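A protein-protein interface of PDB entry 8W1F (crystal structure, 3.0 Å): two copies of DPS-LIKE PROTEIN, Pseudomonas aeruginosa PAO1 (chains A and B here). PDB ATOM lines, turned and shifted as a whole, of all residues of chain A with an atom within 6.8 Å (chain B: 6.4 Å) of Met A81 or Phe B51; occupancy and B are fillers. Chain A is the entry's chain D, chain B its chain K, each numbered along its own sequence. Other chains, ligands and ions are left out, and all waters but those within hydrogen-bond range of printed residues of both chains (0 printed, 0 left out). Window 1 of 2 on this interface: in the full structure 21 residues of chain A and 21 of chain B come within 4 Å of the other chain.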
ATOM      1  N   LEU A  44     -19.778  16.377 -33.296  1.00  0.00           N
ATOM      2  CA  LEU A  44     -18.762  16.181 -32.271  1.00  0.00           C
ATOM      3  C   LEU A  44     -18.552  17.457 -31.478  1.00  0.00           C
ATOM      4  O   LEU A  44     -18.408  17.419 -30.248  1.00  0.00           O
ATOM      5  CB  LEU A  44     -17.457  15.737 -32.916  1.00  0.00           C
ATOM      6  CG  LEU A  44     -16.247  15.676 -31.984  1.00  0.00           C
ATOM      7  CD1 LEU A  44     -16.481  14.735 -30.813  1.00  0.00           C
ATOM      8  CD2 LEU A  44     -15.022  15.319 -32.797  1.00  0.00           C
ATOM      9  N   GLU A  47     -21.526  17.965 -29.176  1.00  0.00           N
ATOM     10  CA  GLU A  47     -21.493  17.125 -27.984  1.00  0.00           C
ATOM     11  C   GLU A  47     -20.495  17.650 -26.960  1.00  0.00           C
ATOM     12  O   GLU A  47     -20.769  17.621 -25.754  1.00  0.00           O
ATOM     13  CB  GLU A  47     -21.175  15.687 -28.374  1.00  0.00           C
ATOM     14  CG  GLU A  47     -22.168  15.119 -29.382  1.00  0.00           C
ATOM     15  CD  GLU A  47     -23.584  15.050 -28.842  1.00  0.00           C
ATOM     16  OE1 GLU A  47     -23.762  14.609 -27.696  1.00  0.00           O
ATOM     17  OE2 GLU A  47     -24.519  15.493 -29.549  1.00  0.00           O
ATOM     18  N   LEU A  48     -19.331  18.113 -27.414  1.00  0.00           N
ATOM     19  CA  LEU A  48     -18.330  18.624 -26.482  1.00  0.00           C
ATOM     20  C   LEU A  48     -18.805  19.895 -25.785  1.00  0.00           C
ATOM     21  O   LEU A  48     -18.602  20.060 -24.578  1.00  0.00           O
ATOM     22  CB  LEU A  48     -17.005  18.870 -27.207  1.00  0.00           C
ATOM     23  CG  LEU A  48     -16.301  17.611 -27.721  1.00  0.00           C
ATOM     24  CD1 LEU A  48     -15.066  17.994 -28.545  1.00  0.00           C
ATOM     25  CD2 LEU A  48     -15.949  16.667 -26.576  1.00  0.00           C
ATOM     26  N   PHE A  51     -21.309  18.870 -23.280  1.00  0.00           N
ATOM     27  CA  PHE A  51     -20.605  18.301 -22.130  1.00  0.00           C
ATOM     28  C   PHE A  51     -20.110  19.390 -21.180  1.00  0.00           C
ATOM     29  O   PHE A  51     -20.261  19.292 -19.955  1.00  0.00           O
ATOM     30  CB  PHE A  51     -19.423  17.464 -22.604  1.00  0.00           C
ATOM     31  CG  PHE A  51     -18.520  17.028 -21.504  1.00  0.00           C
ATOM     32  CD1 PHE A  51     -18.810  15.898 -20.768  1.00  0.00           C
ATOM     33  CD2 PHE A  51     -17.393  17.757 -21.186  1.00  0.00           C
ATOM     34  CE1 PHE A  51     -17.978  15.497 -19.749  1.00  0.00           C
ATOM     35  CE2 PHE A  51     -16.557  17.355 -20.164  1.00  0.00           C
ATOM     36  CZ  PHE A  51     -16.844  16.228 -19.450  1.00  0.00           C
ATOM     37  N   HIS A  76     -26.327  13.469 -17.896  1.00  0.00           N
ATOM     38  CA  HIS A  76     -26.397  13.910 -19.278  1.00  0.00           C
ATOM     39  C   HIS A  76     -25.020  14.316 -19.786  1.00  0.00           C
ATOM     40  O   HIS A  76     -24.642  13.973 -20.909  1.00  0.00           O
ATOM     41  CB  HIS A  76     -27.395  15.063 -19.404  1.00  0.00           C
ATOM     42  CG  HIS A  76     -28.814  14.663 -19.163  1.00  0.00           C
ATOM     43  ND1 HIS A  76     -29.875  15.497 -19.434  1.00  0.00           N
ATOM     44  CD2 HIS A  76     -29.346  13.521 -18.664  1.00  0.00           C
ATOM     45  CE1 HIS A  76     -31.004  14.882 -19.125  1.00  0.00           C
ATOM     46  NE2 HIS A  76     -30.710  13.681 -18.655  1.00  0.00           N
ATOM     47  N   ALA A  77     -24.253  15.042 -18.972  1.00  0.00           N
ATOM     48  CA  ALA A  77     -22.916  15.446 -19.390  1.00  0.00           C
ATOM     49  C   ALA A  77     -22.114  14.245 -19.873  1.00  0.00           C
ATOM     50  O   ALA A  77     -21.509  14.271 -20.951  1.00  0.00           O
ATOM     51  CB  ALA A  77     -22.181  16.128 -18.232  1.00  0.00           C
ATOM     52  N   ASN A  78     -22.090  13.179 -19.078  1.00  0.00           N
ATOM     53  CA  ASN A  78     -21.291  12.038 -19.480  1.00  0.00           C
ATOM     54  C   ASN A  78     -21.914  11.293 -20.655  1.00  0.00           C
ATOM     55  O   ASN A  78     -21.183  10.757 -21.495  1.00  0.00           O
ATOM     56  CB  ASN A  78     -21.070  11.106 -18.299  1.00  0.00           C
ATOM     57  CG  ASN A  78     -20.239  11.742 -17.207  1.00  0.00           C
ATOM     58  OD1 ASN A  78     -19.331  12.564 -17.462  1.00  0.00           O
ATOM     59  ND2 ASN A  78     -20.494  11.314 -15.977  1.00  0.00           N
ATOM     60  N   GLN A  79     -23.238  11.271 -20.768  1.00  0.00           N
ATOM     61  CA  GLN A  79     -23.838  10.710 -21.975  1.00  0.00           C
ATOM     62  C   GLN A  79     -23.452  11.527 -23.209  1.00  0.00           C
ATOM     63  O   GLN A  79     -23.272  10.971 -24.298  1.00  0.00           O
ATOM     64  CB  GLN A  79     -25.350  10.627 -21.823  1.00  0.00           C
ATOM     65  CG  GLN A  79     -25.783   9.451 -20.973  1.00  0.00           C
ATOM     66  CD  GLN A  79     -27.194   9.576 -20.435  1.00  0.00           C
ATOM     67  OE1 GLN A  79     -27.889  10.557 -20.683  1.00  0.00           O
ATOM     68  NE2 GLN A  79     -27.626   8.572 -19.702  1.00  0.00           N
ATOM     69  N   GLU A  80     -23.337  12.850 -23.071  1.00  0.00           N
ATOM     70  CA  GLU A  80     -22.867  13.651 -24.198  1.00  0.00           C
ATOM     71  C   GLU A  80     -21.453  13.241 -24.604  1.00  0.00           C
ATOM     72  O   GLU A  80     -21.116  13.220 -25.796  1.00  0.00           O
ATOM     73  CB  GLU A  80     -22.892  15.146 -23.871  1.00  0.00           C
ATOM     74  CG  GLU A  80     -24.248  15.689 -23.452  1.00  0.00           C
ATOM     75  CD  GLU A  80     -25.358  15.345 -24.426  1.00  0.00           C
ATOM     76  OE1 GLU A  80     -25.166  15.518 -25.646  1.00  0.00           O
ATOM     77  OE2 GLU A  80     -26.437  14.912 -23.970  1.00  0.00           O
ATOM     78  N   MET A  81     -20.604  12.932 -23.623  1.00  0.00           N
ATOM     79  CA  MET A  81     -19.248  12.530 -23.963  1.00  0.00           C
ATOM     80  C   MET A  81     -19.223  11.183 -24.671  1.00  0.00           C
ATOM     81  O   MET A  81     -18.375  10.977 -25.550  1.00  0.00           O
ATOM     82  CB  MET A  81     -18.384  12.483 -22.714  1.00  0.00           C
ATOM     83  CG  MET A  81     -16.916  12.454 -23.039  1.00  0.00           C
ATOM     84  SD  MET A  81     -16.280  14.053 -23.564  1.00  0.00           S
ATOM     85  CE  MET A  81     -15.133  13.443 -24.800  1.00  0.00           C
ATOM     86  N   GLN A  82     -20.124  10.259 -24.311  1.00  0.00           N
ATOM     87  CA  GLN A  82     -20.228   9.020 -25.072  1.00  0.00           C
ATOM     88  C   GLN A  82     -20.600   9.303 -26.519  1.00  0.00           C
ATOM     89  O   GLN A  82     -19.993   8.752 -27.445  1.00  0.00           O
ATOM     90  CB  GLN A  82     -21.241   8.074 -24.443  1.00  0.00           C
ATOM     91  CG  GLN A  82     -20.772   7.396 -23.168  1.00  0.00           C
ATOM     92  CD  GLN A  82     -21.912   6.781 -22.333  1.00  0.00           C
ATOM     93  OE1 GLN A  82     -23.096   6.880 -22.681  1.00  0.00           O
ATOM     94  NE2 GLN A  82     -21.543   6.098 -21.254  1.00  0.00           N
ATOM     95  N   HIS A  83     -21.558  10.202 -26.742  1.00  0.00           N
ATOM     96  CA  HIS A  83     -21.877  10.567 -28.113  1.00  0.00           C
ATOM     97  C   HIS A  83     -20.645  11.116 -28.825  1.00  0.00           C
ATOM     98  O   HIS A  83     -20.387  10.776 -29.987  1.00  0.00           O
ATOM     99  CB  HIS A  83     -23.006  11.599 -28.144  1.00  0.00           C
ATOM    100  CG  HIS A  83     -24.260  11.150 -27.461  1.00  0.00           C
ATOM    101  ND1 HIS A  83     -25.216  12.035 -27.013  1.00  0.00           N
ATOM    102  CD2 HIS A  83     -24.717   9.914 -27.159  1.00  0.00           C
ATOM    103  CE1 HIS A  83     -26.205  11.363 -26.456  1.00  0.00           C
ATOM    104  NE2 HIS A  83     -25.927  10.074 -26.528  1.00  0.00           N
ATOM    105  N   ALA A  84     -19.863  11.953 -28.138  1.00  0.00           N
ATOM    106  CA  ALA A  84     -18.665  12.507 -28.757  1.00  0.00           C
ATOM    107  C   ALA A  84     -17.732  11.397 -29.196  1.00  0.00           C
ATOM    108  O   ALA A  84     -17.205  11.424 -30.313  1.00  0.00           O
ATOM    109  CB  ALA A  84     -17.949  13.461 -27.799  1.00  0.00           C
ATOM    110  N   ASP A  85     -17.512  10.409 -28.319  1.00  0.00           N
ATOM    111  CA  ASP A  85     -16.630   9.295 -28.657  1.00  0.00           C
ATOM    112  C   ASP A  85     -17.187   8.489 -29.818  1.00  0.00           C
ATOM    113  O   ASP A  85     -16.462   8.135 -30.757  1.00  0.00           O
ATOM    114  CB  ASP A  85     -16.450   8.386 -27.440  1.00  0.00           C
ATOM    115  CG  ASP A  85     -15.553   8.984 -26.375  1.00  0.00           C
ATOM    116  OD1 ASP A  85     -14.880  10.010 -26.666  1.00  0.00           O
ATOM    117  OD2 ASP A  85     -15.511   8.400 -25.262  1.00  0.00           O
ATOM    118  N   GLN A  86     -18.490   8.230 -29.776  1.00  0.00           N
ATOM    119  CA  GLN A  86     -19.162   7.455 -30.805  1.00  0.00           C
ATOM    120  C   GLN A  86     -18.984   8.093 -32.164  1.00  0.00           C
ATOM    121  O   GLN A  86     -18.708   7.402 -33.153  1.00  0.00           O
ATOM    122  CB  GLN A  86     -20.630   7.363 -30.405  1.00  0.00           C
ATOM    123  CG  GLN A  86     -21.430   6.234 -30.967  1.00  0.00           C
ATOM    124  CD  GLN A  86     -22.790   6.107 -30.274  1.00  0.00           C
ATOM    125  OE1 GLN A  86     -23.047   6.716 -29.214  1.00  0.00           O
ATOM    126  NE2 GLN A  86     -23.680   5.333 -30.886  1.00  0.00           N
ATOM    127  N   PHE A 100     -11.094  18.096 -31.962  1.00  0.00           N
ATOM    128  CA  PHE A 100     -11.324  18.407 -30.561  1.00  0.00           C
ATOM    129  C   PHE A 100     -10.764  19.774 -30.174  1.00  0.00           C
ATOM    130  O   PHE A 100     -10.572  20.042 -28.981  1.00  0.00           O
ATOM    131  CB  PHE A 100     -10.678  17.355 -29.644  1.00  0.00           C
ATOM    132  CG  PHE A 100     -11.314  15.981 -29.684  1.00  0.00           C
ATOM    133  CD1 PHE A 100     -11.100  15.131 -30.751  1.00  0.00           C
ATOM    134  CD2 PHE A 100     -12.093  15.537 -28.637  1.00  0.00           C
ATOM    135  CE1 PHE A 100     -11.658  13.874 -30.776  1.00  0.00           C
ATOM    136  CE2 PHE A 100     -12.655  14.281 -28.662  1.00  0.00           C
ATOM    137  CZ  PHE A 100     -12.433  13.451 -29.736  1.00  0.00           C
ATOM    138  N   THR B  46      -6.181  24.129 -17.766  1.00  0.00           N
ATOM    139  CA  THR B  46      -5.102  23.260 -18.227  1.00  0.00           C
ATOM    140  C   THR B  46      -5.576  21.811 -18.357  1.00  0.00           C
ATOM    141  O   THR B  46      -5.297  21.139 -19.356  1.00  0.00           O
ATOM    142  CB  THR B  46      -3.913  23.350 -17.261  1.00  0.00           C
ATOM    143  OG1 THR B  46      -3.443  24.698 -17.176  1.00  0.00           O
ATOM    144  CG2 THR B  46      -2.763  22.475 -17.719  1.00  0.00           C
ATOM    145  N   GLU B  47      -6.306  21.310 -17.361  1.00  0.00           N
ATOM    146  CA  GLU B  47      -6.732  19.916 -17.414  1.00  0.00           C
ATOM    147  C   GLU B  47      -7.682  19.671 -18.582  1.00  0.00           C
ATOM    148  O   GLU B  47      -7.577  18.653 -19.268  1.00  0.00           O
ATOM    149  CB  GLU B  47      -7.397  19.516 -16.099  1.00  0.00           C
ATOM    150  CG  GLU B  47      -6.532  19.732 -14.862  1.00  0.00           C
ATOM    151  CD  GLU B  47      -5.241  18.921 -14.857  1.00  0.00           C
ATOM    152  OE1 GLU B  47      -5.264  17.743 -15.241  1.00  0.00           O
ATOM    153  OE2 GLU B  47      -4.199  19.456 -14.437  1.00  0.00           O
ATOM    154  N   LEU B  48      -8.611  20.597 -18.826  1.00  0.00           N
ATOM    155  CA  LEU B  48      -9.552  20.432 -19.931  1.00  0.00           C
ATOM    156  C   LEU B  48      -8.841  20.445 -21.281  1.00  0.00           C
ATOM    157  O   LEU B  48      -9.162  19.634 -22.161  1.00  0.00           O
ATOM    158  CB  LEU B  48     -10.613  21.531 -19.870  1.00  0.00           C
ATOM    159  CG  LEU B  48     -11.539  21.450 -18.661  1.00  0.00           C
ATOM    160  CD1 LEU B  48     -12.412  22.679 -18.574  1.00  0.00           C
ATOM    161  CD2 LEU B  48     -12.428  20.219 -18.705  1.00  0.00           C
ATOM    162  N   VAL B  49      -7.880  21.360 -21.470  1.00  0.00           N
ATOM    163  CA  VAL B  49      -7.094  21.385 -22.706  1.00  0.00           C
ATOM    164  C   VAL B  49      -6.321  20.078 -22.865  1.00  0.00           C
ATOM    165  O   VAL B  49      -6.324  19.464 -23.937  1.00  0.00           O
ATOM    166  CB  VAL B  49      -6.146  22.598 -22.719  1.00  0.00           C
ATOM    167  CG1 VAL B  49      -5.157  22.523 -23.861  1.00  0.00           C
ATOM    168  CG2 VAL B  49      -6.926  23.865 -22.846  1.00  0.00           C
ATOM    169  N   CYS B  50      -5.645  19.631 -21.796  1.00  0.00           N
ATOM    170  CA  CYS B  50      -4.886  18.381 -21.877  1.00  0.00           C
ATOM    171  C   CYS B  50      -5.814  17.195 -22.144  1.00  0.00           C
ATOM    172  O   CYS B  50      -5.440  16.260 -22.855  1.00  0.00           O
ATOM    173  CB  CYS B  50      -4.054  18.159 -20.603  1.00  0.00           C
ATOM    174  SG  CYS B  50      -2.556  19.241 -20.414  1.00  0.00           S
ATOM    175  N   PHE B  51      -7.027  17.216 -21.599  1.00  0.00           N
ATOM    176  CA  PHE B  51      -7.998  16.180 -21.935  1.00  0.00           C
ATOM    177  C   PHE B  51      -8.296  16.162 -23.431  1.00  0.00           C
ATOM    178  O   PHE B  51      -8.334  15.098 -24.064  1.00  0.00           O
ATOM    179  CB  PHE B  51      -9.291  16.396 -21.163  1.00  0.00           C
ATOM    180  CG  PHE B  51     -10.422  15.530 -21.630  1.00  0.00           C
ATOM    181  CD1 PHE B  51     -10.548  14.237 -21.177  1.00  0.00           C
ATOM    182  CD2 PHE B  51     -11.347  16.002 -22.527  1.00  0.00           C
ATOM    183  CE1 PHE B  51     -11.573  13.451 -21.605  1.00  0.00           C
ATOM    184  CE2 PHE B  51     -12.378  15.209 -22.946  1.00  0.00           C
ATOM    185  CZ  PHE B  51     -12.489  13.940 -22.490  1.00  0.00           C
ATOM    186  N   LEU B  52      -8.553  17.336 -24.005  1.00  0.00           N
ATOM    187  CA  LEU B  52      -8.892  17.401 -25.420  1.00  0.00           C
ATOM    188  C   LEU B  52      -7.722  16.970 -26.297  1.00  0.00           C
ATOM    189  O   LEU B  52      -7.924  16.249 -27.279  1.00  0.00           O
ATOM    190  CB  LEU B  52      -9.369  18.808 -25.771  1.00  0.00           C
ATOM    191  CG  LEU B  52     -10.685  19.242 -25.119  1.00  0.00           C
ATOM    192  CD1 LEU B  52     -10.849  20.719 -25.342  1.00  0.00           C
ATOM    193  CD2 LEU B  52     -11.856  18.485 -25.688  1.00  0.00           C
ATOM    194  N   ARG B  53      -6.491  17.400 -25.970  1.00  0.00           N
ATOM    195  CA  ARG B  53      -5.321  16.968 -26.742  1.00  0.00           C
ATOM    196  C   ARG B  53      -5.186  15.450 -26.750  1.00  0.00           C
ATOM    197  O   ARG B  53      -5.034  14.828 -27.807  1.00  0.00           O
ATOM    198  CB  ARG B  53      -4.041  17.563 -26.162  1.00  0.00           C
ATOM    199  CG  ARG B  53      -2.994  17.923 -27.207  1.00  0.00           C
ATOM    200  CD  ARG B  53      -1.588  18.013 -26.604  1.00  0.00           C
ATOM    201  NE  ARG B  53      -1.598  18.785 -25.369  1.00  0.00           N
ATOM    202  CZ  ARG B  53      -1.502  18.272 -24.151  1.00  0.00           C
ATOM    203  NH1 ARG B  53      -1.253  16.987 -23.953  1.00  0.00           N
ATOM    204  NH2 ARG B  53      -1.657  19.075 -23.103  1.00  0.00           N
ATOM    205  N   TYR B  54      -5.232  14.836 -25.571  1.00  0.00           N
ATOM    206  CA  TYR B  54      -5.019  13.399 -25.486  1.00  0.00           C
ATOM    207  C   TYR B  54      -6.111  12.637 -26.228  1.00  0.00           C
ATOM    208  O   TYR B  54      -5.845  11.590 -26.823  1.00  0.00           O
ATOM    209  CB  TYR B  54      -4.956  12.962 -24.023  1.00  0.00           C
ATOM    210  CG  TYR B  54      -3.579  13.001 -23.366  1.00  0.00           C
ATOM    211  CD1 TYR B  54      -2.527  12.245 -23.850  1.00  0.00           C
ATOM    212  CD2 TYR B  54      -3.362  13.751 -22.219  1.00  0.00           C
ATOM    213  CE1 TYR B  54      -1.285  12.258 -23.232  1.00  0.00           C
ATOM    214  CE2 TYR B  54      -2.139  13.764 -21.596  1.00  0.00           C
ATOM    215  CZ  TYR B  54      -1.100  13.015 -22.104  1.00  0.00           C
ATOM    216  OH  TYR B  54       0.137  13.012 -21.490  1.00  0.00           O
ATOM    217  N   LYS B  55      -7.354  13.112 -26.169  1.00  0.00           N
ATOM    218  CA  LYS B  55      -8.416  12.431 -26.906  1.00  0.00           C
ATOM    219  C   LYS B  55      -8.145  12.479 -28.406  1.00  0.00           C
ATOM    220  O   LYS B  55      -8.255  11.465 -29.106  1.00  0.00           O
ATOM    221  CB  LYS B  55      -9.760  13.079 -26.589  1.00  0.00           C
ATOM    222  CG  LYS B  55     -10.336  12.690 -25.233  1.00  0.00           C
ATOM    223  CD  LYS B  55     -10.774  11.253 -25.166  1.00  0.00           C
ATOM    224  CE  LYS B  55     -12.255  11.148 -25.458  1.00  0.00           C
ATOM    225  NZ  LYS B  55     -12.717   9.783 -25.081  1.00  0.00           N
ATOM    226  N   ARG B  56      -7.741  13.645 -28.909  1.00  0.00           N
ATOM    227  CA  ARG B  56      -7.341  13.751 -30.307  1.00  0.00           C
ATOM    228  C   ARG B  56      -6.261  12.725 -30.618  1.00  0.00           C
ATOM    229  O   ARG B  56      -6.370  11.960 -31.584  1.00  0.00           O
ATOM    230  CB  ARG B  56      -6.856  15.176 -30.598  1.00  0.00           C
ATOM    231  CG  ARG B  56      -6.056  15.365 -31.880  1.00  0.00           C
ATOM    232  CD  ARG B  56      -6.922  15.305 -33.120  1.00  0.00           C
ATOM    233  NE  ARG B  56      -6.141  15.501 -34.335  1.00  0.00           N
ATOM    234  CZ  ARG B  56      -6.658  15.858 -35.503  1.00  0.00           C
ATOM    235  NH1 ARG B  56      -7.949  16.104 -35.640  1.00  0.00           N
ATOM    236  NH2 ARG B  56      -5.855  16.006 -36.551  1.00  0.00           N
ATOM    237  N   HIS B  76      -4.428   8.649 -19.873  1.00  0.00           N
ATOM    238  CA  HIS B  76      -4.089   9.966 -19.360  1.00  0.00           C
ATOM    239  C   HIS B  76      -5.240  10.938 -19.541  1.00  0.00           C
ATOM    240  O   HIS B  76      -5.572  11.683 -18.617  1.00  0.00           O
ATOM    241  CB  HIS B  76      -2.822  10.494 -20.032  1.00  0.00           C
ATOM    242  CG  HIS B  76      -1.591   9.739 -19.654  1.00  0.00           C
ATOM    243  ND1 HIS B  76      -0.325  10.184 -19.955  1.00  0.00           N
ATOM    244  CD2 HIS B  76      -1.434   8.555 -19.013  1.00  0.00           C
ATOM    245  CE1 HIS B  76       0.561   9.316 -19.498  1.00  0.00           C
ATOM    246  NE2 HIS B  76      -0.086   8.318 -18.924  1.00  0.00           N
ATOM    247  N   ALA B  77      -5.883  10.925 -20.706  1.00  0.00           N
ATOM    248  CA  ALA B  77      -6.987  11.852 -20.931  1.00  0.00           C
ATOM    249  C   ALA B  77      -7.992  11.771 -19.793  1.00  0.00           C
ATOM    250  O   ALA B  77      -8.381  12.789 -19.207  1.00  0.00           O
ATOM    251  CB  ALA B  77      -7.682  11.553 -22.264  1.00  0.00           C
ATOM    252  N   ASN B  78      -8.404  10.556 -19.445  1.00  0.00           N
ATOM    253  CA  ASN B  78      -9.418  10.431 -18.417  1.00  0.00           C
ATOM    254  C   ASN B  78      -8.879  10.795 -17.033  1.00  0.00           C
ATOM    255  O   ASN B  78      -9.627  11.335 -16.207  1.00  0.00           O
ATOM    256  CB  ASN B  78     -10.003   9.018 -18.442  1.00  0.00           C
ATOM    257  CG  ASN B  78     -10.784   8.735 -19.713  1.00  0.00           C
ATOM    258  OD1 ASN B  78     -11.437   9.625 -20.276  1.00  0.00           O
ATOM    259  ND2 ASN B  78     -10.769   7.479 -20.141  1.00  0.00           N
ATOM    260  N   GLU B  80      -6.804  13.201 -16.617  1.00  0.00           N
ATOM    261  CA  GLU B  80      -6.879  14.654 -16.648  1.00  0.00           C
ATOM    262  C   GLU B  80      -8.271  15.128 -16.261  1.00  0.00           C
ATOM    263  O   GLU B  80      -8.423  16.091 -15.505  1.00  0.00           O
ATOM    264  CB  GLU B  80      -6.529  15.197 -18.030  1.00  0.00           C
ATOM    265  CG  GLU B  80      -5.155  14.809 -18.553  1.00  0.00           C
ATOM    266  CD  GLU B  80      -4.032  15.091 -17.567  1.00  0.00           C
ATOM    267  OE1 GLU B  80      -4.250  15.832 -16.589  1.00  0.00           O
ATOM    268  OE2 GLU B  80      -2.906  14.601 -17.803  1.00  0.00           O
ATOM    269  N   MET B  81      -9.302  14.440 -16.744  1.00  0.00           N
ATOM    270  CA  MET B  81     -10.652  14.859 -16.409  1.00  0.00           C
ATOM    271  C   MET B  81     -10.934  14.654 -14.925  1.00  0.00           C
ATOM    272  O   MET B  81     -11.644  15.465 -14.322  1.00  0.00           O
ATOM    273  CB  MET B  81     -11.658  14.109 -17.279  1.00  0.00           C
ATOM    274  CG  MET B  81     -13.035  14.765 -17.322  1.00  0.00           C
ATOM    275  SD  MET B  81     -13.099  16.225 -18.380  1.00  0.00           S
ATOM    276  CE  MET B  81     -14.163  17.211 -17.310  1.00  0.00           C
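Phe A51 touches Met B81, and with the chains exchanged Met A81 touches Phe B51. Positions printed for both chains: 47, 48, 51, 76, 77, 78, 80 and 81. Of the 6 pairs that touch across the chains among the printed residues, 2 have their exchanged pair printed and touching as well.
The side-chain carboxylate of Asp A85 lies within salt-bridge range of the side-chain amino group of Lys B55.
Along chain B the printed residues that touch a printed residue of chain A span positions 51 to 81. Of the 16 printed residues of chain A, 4 touch a printed residue of chain B. Among the printed residues, 6 pairs touch across the chains.
Gln A79 touches none of the printed residues of chain B. Printed residues of chain B within 4 Å of Met A81: Phe B51 (3.5 Å) and Lys B55 (3.7 Å). Of the printed residues of chain B, Phe A100 touches Leu B52 (3.6 Å) and Lys B55 (3.8 Å). Of chain A, only Met A81 (3.5 Å) comes within 4 Å of Phe B51. Printed residues of chain A within 4 Å of Lys B55: Met A81 (3.7 Å), Asp A85 (2.7 Å) and Phe A100 (3.8 Å). Asn B78 touches none of the printed residues of chain A. Of the printed residues of chain A, Met B81 touches Phe A51 (3.6 Å). The nearest residue of chain B that does not touch Met A81 is Leu B52 (6.1 Å). The nearest printed residue of chain B that does not touch Phe A51 is Leu B48 (5.2 Å).
CZ of Phe A51 touches CE of Met B81 (3.6 Å). Met A81 touches Phe B51. CE of Met A81 touches CE of Lys B55, 3.7 Å away. Leu B52 touches Phe A100. Phe A100 touches Lys B55 (CE2 to CB, 3.8 Å).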
